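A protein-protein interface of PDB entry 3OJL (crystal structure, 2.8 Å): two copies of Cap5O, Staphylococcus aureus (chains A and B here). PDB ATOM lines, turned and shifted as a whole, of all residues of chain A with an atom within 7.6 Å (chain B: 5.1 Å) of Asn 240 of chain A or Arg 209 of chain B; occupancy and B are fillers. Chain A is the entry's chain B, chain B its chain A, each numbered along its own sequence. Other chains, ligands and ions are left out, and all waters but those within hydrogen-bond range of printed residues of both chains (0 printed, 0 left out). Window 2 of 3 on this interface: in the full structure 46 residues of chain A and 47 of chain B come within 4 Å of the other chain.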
ATOM      1  N   LYS A 234      32.817  19.392 -10.024  1.00  0.00           N
ATOM      2  CA  LYS A 234      31.784  20.110 -10.755  1.00  0.00           C
ATOM      3  C   LYS A 234      31.173  19.185 -11.803  1.00  0.00           C
ATOM      4  O   LYS A 234      29.946  19.073 -11.852  1.00  0.00           O
ATOM      5  CB  LYS A 234      32.318  21.399 -11.387  1.00  0.00           C
ATOM      6  CG  LYS A 234      32.768  22.449 -10.381  1.00  0.00           C
ATOM      7  CD  LYS A 234      32.883  23.817 -11.054  1.00  0.00           C
ATOM      8  CE  LYS A 234      33.654  24.795 -10.210  1.00  0.00           C
ATOM      9  NZ  LYS A 234      33.576  26.169 -10.761  1.00  0.00           N
ATOM     10  N   ILE A 235      32.015  18.451 -12.558  1.00  0.00           N
ATOM     11  CA  ILE A 235      31.572  17.504 -13.591  1.00  0.00           C
ATOM     12  C   ILE A 235      30.789  16.334 -12.974  1.00  0.00           C
ATOM     13  O   ILE A 235      29.687  16.024 -13.441  1.00  0.00           O
ATOM     14  CB  ILE A 235      32.730  17.036 -14.515  1.00  0.00           C
ATOM     15  CG1 ILE A 235      33.423  18.244 -15.192  1.00  0.00           C
ATOM     16  CG2 ILE A 235      32.216  16.053 -15.564  1.00  0.00           C
ATOM     17  CD1 ILE A 235      34.704  17.956 -15.996  1.00  0.00           C
ATOM     18  N   CYS A 236      31.346  15.714 -11.915  1.00  0.00           N
ATOM     19  CA  CYS A 236      30.783  14.549 -11.233  1.00  0.00           C
ATOM     20  C   CYS A 236      29.436  14.819 -10.645  1.00  0.00           C
ATOM     21  O   CYS A 236      28.560  13.965 -10.751  1.00  0.00           O
ATOM     22  CB  CYS A 236      31.744  14.004 -10.178  1.00  0.00           C
ATOM     23  SG  CYS A 236      33.065  12.973 -10.838  1.00  0.00           S
ATOM     24  N   ASN A 237      29.265  15.994 -10.009  1.00  0.00           N
ATOM     25  CA  ASN A 237      27.998  16.358  -9.369  1.00  0.00           C
ATOM     26  C   ASN A 237      26.856  16.518 -10.380  1.00  0.00           C
ATOM     27  O   ASN A 237      25.728  16.088 -10.098  1.00  0.00           O
ATOM     28  CB  ASN A 237      28.149  17.555  -8.434  1.00  0.00           C
ATOM     29  CG  ASN A 237      28.753  17.198  -7.084  1.00  0.00           C
ATOM     30  OD1 ASN A 237      29.754  17.774  -6.668  1.00  0.00           O
ATOM     31  ND2 ASN A 237      28.159  16.260  -6.344  1.00  0.00           N
ATOM     32  N   ASN A 238      27.182  17.028 -11.592  1.00  0.00           N
ATOM     33  CA  ASN A 238      26.238  17.191 -12.695  1.00  0.00           C
ATOM     34  C   ASN A 238      25.887  15.853 -13.340  1.00  0.00           C
ATOM     35  O   ASN A 238      24.843  15.747 -13.985  1.00  0.00           O
ATOM     36  CB  ASN A 238      26.809  18.135 -13.744  1.00  0.00           C
ATOM     37  CG  ASN A 238      26.779  19.580 -13.326  1.00  0.00           C
ATOM     38  OD1 ASN A 238      26.146  19.955 -12.327  1.00  0.00           O
ATOM     39  ND2 ASN A 238      27.438  20.431 -14.100  1.00  0.00           N
ATOM     40  N   LEU A 239      26.765  14.838 -13.174  1.00  0.00           N
ATOM     41  CA  LEU A 239      26.612  13.511 -13.755  1.00  0.00           C
ATOM     42  C   LEU A 239      26.154  12.481 -12.741  1.00  0.00           C
ATOM     43  O   LEU A 239      25.999  11.320 -13.093  1.00  0.00           O
ATOM     44  CB  LEU A 239      27.932  13.075 -14.399  1.00  0.00           C
ATOM     45  CG  LEU A 239      28.331  13.744 -15.715  1.00  0.00           C
ATOM     46  CD1 LEU A 239      29.693  13.292 -16.142  1.00  0.00           C
ATOM     47  CD2 LEU A 239      27.359  13.431 -16.836  1.00  0.00           C
ATOM     48  N   ASN A 240      25.919  12.901 -11.488  1.00  0.00           N
ATOM     49  CA  ASN A 240      25.478  12.031 -10.384  1.00  0.00           C
ATOM     50  C   ASN A 240      26.467  10.891 -10.091  1.00  0.00           C
ATOM     51  O   ASN A 240      26.067   9.753  -9.833  1.00  0.00           O
ATOM     52  CB  ASN A 240      24.021  11.568 -10.565  1.00  0.00           C
ATOM     53  CG  ASN A 240      23.010  12.594 -10.124  1.00  0.00           C
ATOM     54  OD1 ASN A 240      23.079  13.777 -10.473  1.00  0.00           O
ATOM     55  ND2 ASN A 240      22.079  12.171  -9.283  1.00  0.00           N
ATOM     56  N   ILE A 241      27.770  11.241 -10.112  1.00  0.00           N
ATOM     57  CA  ILE A 241      28.931  10.375  -9.872  1.00  0.00           C
ATOM     58  C   ILE A 241      29.634  10.855  -8.593  1.00  0.00           C
ATOM     59  O   ILE A 241      29.697  12.065  -8.353  1.00  0.00           O
ATOM     60  CB  ILE A 241      29.860  10.401 -11.139  1.00  0.00           C
ATOM     61  CG1 ILE A 241      29.131   9.800 -12.366  1.00  0.00           C
ATOM     62  CG2 ILE A 241      31.190   9.681 -10.906  1.00  0.00           C
ATOM     63  CD1 ILE A 241      29.784  10.037 -13.721  1.00  0.00           C
ATOM     64  N   ASN A 242      30.150   9.921  -7.759  1.00  0.00           N
ATOM     65  CA  ASN A 242      30.852  10.302  -6.513  1.00  0.00           C
ATOM     66  C   ASN A 242      32.310  10.624  -6.815  1.00  0.00           C
ATOM     67  O   ASN A 242      33.094   9.707  -7.044  1.00  0.00           O
ATOM     68  CB  ASN A 242      30.752   9.177  -5.462  1.00  0.00           C
ATOM     69  CG  ASN A 242      31.179   9.565  -4.064  1.00  0.00           C
ATOM     70  OD1 ASN A 242      32.355   9.788  -3.768  1.00  0.00           O
ATOM     71  ND2 ASN A 242      30.234   9.594  -3.175  1.00  0.00           N
ATOM     72  N   VAL A 243      32.675  11.915  -6.820  1.00  0.00           N
ATOM     73  CA  VAL A 243      34.051  12.374  -7.104  1.00  0.00           C
ATOM     74  C   VAL A 243      35.115  11.697  -6.208  1.00  0.00           C
ATOM     75  O   VAL A 243      36.153  11.249  -6.711  1.00  0.00           O
ATOM     76  CB  VAL A 243      34.182  13.926  -7.179  1.00  0.00           C
ATOM     77  CG1 VAL A 243      33.886  14.591  -5.844  1.00  0.00           C
ATOM     78  CG2 VAL A 243      35.544  14.347  -7.698  1.00  0.00           C
ATOM     79  N   VAL A 246      35.649   8.079  -7.183  1.00  0.00           N
ATOM     80  CA  VAL A 246      36.353   8.129  -8.466  1.00  0.00           C
ATOM     81  C   VAL A 246      37.851   8.363  -8.242  1.00  0.00           C
ATOM     82  O   VAL A 246      38.651   7.592  -8.781  1.00  0.00           O
ATOM     83  CB  VAL A 246      35.722   9.161  -9.457  1.00  0.00           C
ATOM     84  CG1 VAL A 246      36.559   9.329 -10.730  1.00  0.00           C
ATOM     85  CG2 VAL A 246      34.287   8.777  -9.806  1.00  0.00           C
ATOM     86  N   GLY A 423      31.010  14.269  -2.976  1.00  0.00           N
ATOM     87  CA  GLY A 423      30.595  13.081  -3.703  1.00  0.00           C
ATOM     88  C   GLY A 423      29.135  12.737  -3.484  1.00  0.00           C
ATOM     89  O   GLY A 423      28.597  11.905  -4.206  1.00  0.00           O
ATOM     90  N   ASN A 424      28.484  13.364  -2.480  1.00  0.00           N
ATOM     91  CA  ASN A 424      27.094  13.109  -2.081  1.00  0.00           C
ATOM     92  C   ASN A 424      26.084  14.217  -2.374  1.00  0.00           C
ATOM     93  O   ASN A 424      24.914  13.883  -2.554  1.00  0.00           O
ATOM     94  CB  ASN A 424      27.002  12.771  -0.585  1.00  0.00           C
ATOM     95  CG  ASN A 424      27.675  11.486  -0.175  1.00  0.00           C
ATOM     96  OD1 ASN A 424      27.411  10.405  -0.711  1.00  0.00           O
ATOM     97  ND2 ASN A 424      28.509  11.565   0.844  1.00  0.00           N
ATOM     98  N   ILE A 425      26.486  15.524  -2.356  1.00  0.00           N
ATOM     99  CA  ILE A 425      25.560  16.664  -2.565  1.00  0.00           C
ATOM    100  C   ILE A 425      24.493  16.537  -3.615  1.00  0.00           C
ATOM    101  O   ILE A 425      23.400  17.066  -3.399  1.00  0.00           O
ATOM    102  CB  ILE A 425      26.140  18.081  -2.614  1.00  0.00           C
ATOM    103  CG1 ILE A 425      27.640  18.114  -2.903  1.00  0.00           C
ATOM    104  CG2 ILE A 425      25.659  18.918  -1.427  1.00  0.00           C
ATOM    105  CD1 ILE A 425      28.077  19.135  -3.939  1.00  0.00           C
ATOM    106  N   PHE A 426      24.790  15.894  -4.756  1.00  0.00           N
ATOM    107  CA  PHE A 426      23.791  15.743  -5.807  1.00  0.00           C
ATOM    108  C   PHE A 426      22.536  14.959  -5.325  1.00  0.00           C
ATOM    109  O   PHE A 426      21.472  15.086  -5.937  1.00  0.00           O
ATOM    110  CB  PHE A 426      24.411  15.145  -7.079  1.00  0.00           C
ATOM    111  CG  PHE A 426      25.055  13.792  -6.896  1.00  0.00           C
ATOM    112  CD1 PHE A 426      24.291  12.630  -6.905  1.00  0.00           C
ATOM    113  CD2 PHE A 426      26.424  13.677  -6.723  1.00  0.00           C
ATOM    114  CE1 PHE A 426      24.885  11.386  -6.723  1.00  0.00           C
ATOM    115  CE2 PHE A 426      27.018  12.429  -6.564  1.00  0.00           C
ATOM    116  CZ  PHE A 426      26.245  11.294  -6.552  1.00  0.00           C
ATOM    117  N   ASN A 427      22.665  14.193  -4.204  1.00  0.00           N
ATOM    118  CA  ASN A 427      21.612  13.381  -3.585  1.00  0.00           C
ATOM    119  C   ASN A 427      20.576  14.202  -2.814  1.00  0.00           C
ATOM    120  O   ASN A 427      19.487  13.691  -2.526  1.00  0.00           O
ATOM    121  CB  ASN A 427      22.198  12.259  -2.708  1.00  0.00           C
ATOM    122  CG  ASN A 427      22.755  11.090  -3.496  1.00  0.00           C
ATOM    123  OD1 ASN A 427      22.285  10.743  -4.595  1.00  0.00           O
ATOM    124  ND2 ASN A 427      23.750  10.428  -2.926  1.00  0.00           N
ATOM    125  N   ILE A 429      18.606  15.925  -3.822  1.00  0.00           N
ATOM    126  CA  ILE A 429      17.724  15.874  -4.994  1.00  0.00           C
ATOM    127  C   ILE A 429      17.956  16.951  -6.087  1.00  0.00           C
ATOM    128  O   ILE A 429      17.336  16.888  -7.158  1.00  0.00           O
ATOM    129  CB  ILE A 429      16.248  15.503  -4.634  1.00  0.00           C
ATOM    130  CG1 ILE A 429      15.773  14.239  -5.394  1.00  0.00           C
ATOM    131  CG2 ILE A 429      15.247  16.673  -4.687  1.00  0.00           C
ATOM    132  CD1 ILE A 429      16.453  12.847  -4.929  1.00  0.00           C
ATOM    133  N   ASP A 430      18.929  17.866  -5.839  1.00  0.00           N
ATOM    134  CA  ASP A 430      19.336  18.956  -6.736  1.00  0.00           C
ATOM    135  C   ASP A 430      20.358  18.497  -7.792  1.00  0.00           C
ATOM    136  O   ASP A 430      20.668  17.308  -7.907  1.00  0.00           O
ATOM    137  CB  ASP A 430      19.890  20.145  -5.922  1.00  0.00           C
ATOM    138  CG  ASP A 430      21.084  19.822  -5.033  1.00  0.00           C
ATOM    139  OD1 ASP A 430      20.986  18.872  -4.226  1.00  0.00           O
ATOM    140  OD2 ASP A 430      22.094  20.552  -5.108  1.00  0.00           O
ATOM    141  N   LYS B 134      28.609   7.694 -17.623  1.00  0.00           N
ATOM    142  CA  LYS B 134      27.155   7.494 -17.666  1.00  0.00           C
ATOM    143  C   LYS B 134      26.650   6.798 -18.932  1.00  0.00           C
ATOM    144  O   LYS B 134      25.443   6.773 -19.141  1.00  0.00           O
ATOM    145  CB  LYS B 134      26.348   8.769 -17.315  1.00  0.00           C
ATOM    146  CG  LYS B 134      26.598   9.314 -15.881  1.00  0.00           C
ATOM    147  CD  LYS B 134      25.725   8.678 -14.768  1.00  0.00           C
ATOM    148  CE  LYS B 134      24.241   9.020 -14.811  1.00  0.00           C
ATOM    149  NZ  LYS B 134      23.965  10.481 -14.940  1.00  0.00           N
ATOM    150  N   ASP B 137      24.583   3.490 -17.892  1.00  0.00           N
ATOM    151  CA  ASP B 137      23.341   3.854 -17.219  1.00  0.00           C
ATOM    152  C   ASP B 137      22.306   4.526 -18.073  1.00  0.00           C
ATOM    153  O   ASP B 137      21.114   4.296 -17.877  1.00  0.00           O
ATOM    154  CB  ASP B 137      23.650   4.773 -16.042  1.00  0.00           C
ATOM    155  CG  ASP B 137      24.671   4.217 -15.105  1.00  0.00           C
ATOM    156  OD1 ASP B 137      25.883   4.481 -15.327  1.00  0.00           O
ATOM    157  OD2 ASP B 137      24.274   3.505 -14.155  1.00  0.00           O
ATOM    158  N   ASP B 207      31.094   0.487  -9.090  1.00  0.00           N
ATOM    159  CA  ASP B 207      29.913   0.568  -9.967  1.00  0.00           C
ATOM    160  C   ASP B 207      30.303   1.090 -11.367  1.00  0.00           C
ATOM    161  O   ASP B 207      31.350   1.730 -11.491  1.00  0.00           O
ATOM    162  CB  ASP B 207      28.797   1.408  -9.344  1.00  0.00           C
ATOM    163  CG  ASP B 207      29.080   2.860  -9.174  1.00  0.00           C
ATOM    164  OD1 ASP B 207      30.189   3.292  -9.537  1.00  0.00           O
ATOM    165  OD2 ASP B 207      28.189   3.571  -8.680  1.00  0.00           O
ATOM    166  N   ALA B 208      29.482   0.820 -12.398  1.00  0.00           N
ATOM    167  CA  ALA B 208      29.726   1.234 -13.776  1.00  0.00           C
ATOM    168  C   ALA B 208      30.233   2.693 -13.917  1.00  0.00           C
ATOM    169  O   ALA B 208      31.353   2.874 -14.391  1.00  0.00           O
ATOM    170  CB  ALA B 208      28.495   0.989 -14.630  1.00  0.00           C
ATOM    171  N   ARG B 209      29.471   3.710 -13.433  1.00  0.00           N
ATOM    172  CA  ARG B 209      29.859   5.122 -13.507  1.00  0.00           C
ATOM    173  C   ARG B 209      31.226   5.484 -12.907  1.00  0.00           C
ATOM    174  O   ARG B 209      31.968   6.279 -13.505  1.00  0.00           O
ATOM    175  CB  ARG B 209      28.740   6.070 -13.056  1.00  0.00           C
ATOM    176  CG  ARG B 209      28.406   6.069 -11.564  1.00  0.00           C
ATOM    177  CD  ARG B 209      27.189   6.929 -11.282  1.00  0.00           C
ATOM    178  NE  ARG B 209      25.950   6.213 -11.573  1.00  0.00           N
ATOM    179  CZ  ARG B 209      24.737   6.753 -11.521  1.00  0.00           C
ATOM    180  NH1 ARG B 209      24.583   8.031 -11.196  1.00  0.00           N
ATOM    181  NH2 ARG B 209      23.668   6.020 -11.792  1.00  0.00           N
ATOM    182  N   THR B 210      31.585   4.866 -11.772  1.00  0.00           N
ATOM    183  CA  THR B 210      32.907   5.079 -11.184  1.00  0.00           C
ATOM    184  C   THR B 210      34.001   4.444 -12.072  1.00  0.00           C
ATOM    185  O   THR B 210      34.996   5.092 -12.328  1.00  0.00           O
ATOM    186  CB  THR B 210      32.949   4.651  -9.710  1.00  0.00           C
ATOM    187  OG1 THR B 210      31.884   5.299  -9.016  1.00  0.00           O
ATOM    188  CG2 THR B 210      34.266   4.990  -9.036  1.00  0.00           C
ATOM    189  N   ALA B 211      33.794   3.225 -12.571  1.00  0.00           N
ATOM    190  CA  ALA B 211      34.754   2.538 -13.425  1.00  0.00           C
ATOM    191  C   ALA B 211      35.016   3.316 -14.718  1.00  0.00           C
ATOM    192  O   ALA B 211      36.173   3.380 -15.173  1.00  0.00           O
ATOM    193  CB  ALA B 211      34.255   1.148 -13.739  1.00  0.00           C
ATOM    194  N   GLU B 212      33.941   3.942 -15.286  1.00  0.00           N
ATOM    195  CA  GLU B 212      33.997   4.791 -16.480  1.00  0.00           C
ATOM    196  C   GLU B 212      34.743   6.083 -16.170  1.00  0.00           C
ATOM    197  O   GLU B 212      35.673   6.424 -16.884  1.00  0.00           O
ATOM    198  CB  GLU B 212      32.582   5.149 -16.979  1.00  0.00           C
ATOM    199  CG  GLU B 212      31.728   3.985 -17.441  1.00  0.00           C
ATOM    200  CD  GLU B 212      30.251   4.288 -17.578  1.00  0.00           C
ATOM    201  OE1 GLU B 212      29.651   3.783 -18.548  1.00  0.00           O
ATOM    202  OE2 GLU B 212      29.682   4.991 -16.713  1.00  0.00           O
ATOM    203  N   MET B 213      34.325   6.818 -15.124  1.00  0.00           N
ATOM    204  CA  MET B 213      34.936   8.103 -14.748  1.00  0.00           C
ATOM    205  C   MET B 213      36.396   7.946 -14.328  1.00  0.00           C
ATOM    206  O   MET B 213      37.244   8.661 -14.853  1.00  0.00           O
ATOM    207  CB  MET B 213      34.081   8.850 -13.698  1.00  0.00           C
ATOM    208  CG  MET B 213      34.388  10.359 -13.554  1.00  0.00           C
ATOM    209  SD  MET B 213      34.693  11.294 -15.073  1.00  0.00           S
ATOM    210  CE  MET B 213      33.381  12.508 -14.993  1.00  0.00           C
ATOM    211  N   SER B 214      36.687   6.962 -13.462  1.00  0.00           N
ATOM    212  CA  SER B 214      38.025   6.594 -12.975  1.00  0.00           C
ATOM    213  C   SER B 214      39.001   6.306 -14.089  1.00  0.00           C
ATOM    214  O   SER B 214      40.125   6.802 -14.020  1.00  0.00           O
ATOM    215  CB  SER B 214      37.963   5.351 -12.084  1.00  0.00           C
ATOM    216  OG  SER B 214      37.082   5.555 -10.988  1.00  0.00           O
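No position is printed for both chains. Of the 10 pairs that touch across the chains among the printed residues, none has its exchanged pair printed and touching as well.
Asn 240 of chain A touches just one residue of chain B: Arg 209. Of chain A, only Asn 240 (2.7 Å) and Ile 241 (3.6 Å) come within 4 Å of Arg 209 of chain B. Printed residues of chain B within 4 Å of Cys 236 of chain A: Met 213. Of the printed residues of chain B, Val 246 of chain A touches Thr 210, Met 213 and Ser 214. Of the printed residues of chain B, Ile 235 of chain A touches Met 213 (3.8 Å). Of the printed residues of chain A, Met 213 of chain B touches Ile 235 (3.8 Å), Cys 236 (3.99 Å), Leu 239 (3.9 Å) and Val 246 (3.7 Å). Asn 238 of chain A touches none of the printed residues of chain B. The nearest residue of chain A that does not touch Arg 209 of chain B is Leu 239 of chain A (4.1 Å). The nearest printed residue of chain B that does not touch Ile 241 of chain A is Met 213 of chain B (4.1 Å).
Hydrophobic or aromatic side chains of chain B that line the printed part of chain A: Met 213. Along chain B the printed residues that touch a printed residue of chain A span positions 134 to 214. Of the 18 printed residues of chain A, 6 touch a printed residue of chain B. Printed residues of chain A that touch a printed residue of chain B: Ile 235, Cys 236, Leu 239, Asn 240, Ile 241 and Val 246. Hydrophobic or aromatic side chains of chain A within 4 Å of the printed part of chain B: Ile 235, Leu 239, Ile 241 and Val 246. Among the printed residues, 10 pairs touch across the chains.
O of Leu 239 of chain A is in hydrogen-bond range of NZ of Lys 134 of chain B, 2.9 Å away. The guanidinium group (NH1) of Arg 209 of chain B is in hydrogen-bond range of the backbone carbonyl oxygen (O) of Asn 240 of chain A, 2.7 Å away. OG of Ser 214 of chain B is in hydrogen-bond range of O of Val 246 of chain A (3.4 Å).
CG2 of Ile 235 of chain A touches CE of Met 213 of chain B (3.8 Å). SG of Cys 236 of chain A touches CG of Met 213 of chain B (3.99 Å). Met 213 of chain B touches Leu 239 of chain A (CE to CD1, 3.9 Å). Ile 241 of chain A touches Lys 134 of chain B. Arg 209 of chain B touches Ile 241 of chain A (CD to CG1, 3.6 Å). CG2 of Thr 210 of chain B touches CA of Val 246 of chain A (3.8 Å). CG1 of Val 246 of chain A touches CG of Met 213 of chain B (3.7 Å).
OE2 of Glu 212 of chain B sits at hydrogen-bond distance from N of Lys 134 of chain B (3.0 Å). The guanidinium group (NH2) of Arg 209 of chain B is in salt-bridge range of the side-chain carboxylate (OD2) of Asp 137 of chain B (3.5 Å). The side-chain carboxylate (OD1) of Asp 207 of chain B is in hydrogen-bond range of the side-chain hydroxyl (OG1) of Thr 210 of chain B (2.7 Å). O of Thr 210 of chain B lies within hydrogen-bond range of OG of Ser 214 of chain B, 2.5 Å away. The backbone carbonyl oxygen of Cys 236 of chain A is in hydrogen-bond range of the backbone NH of Ile 241 of chain A, at 2.9 Å.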
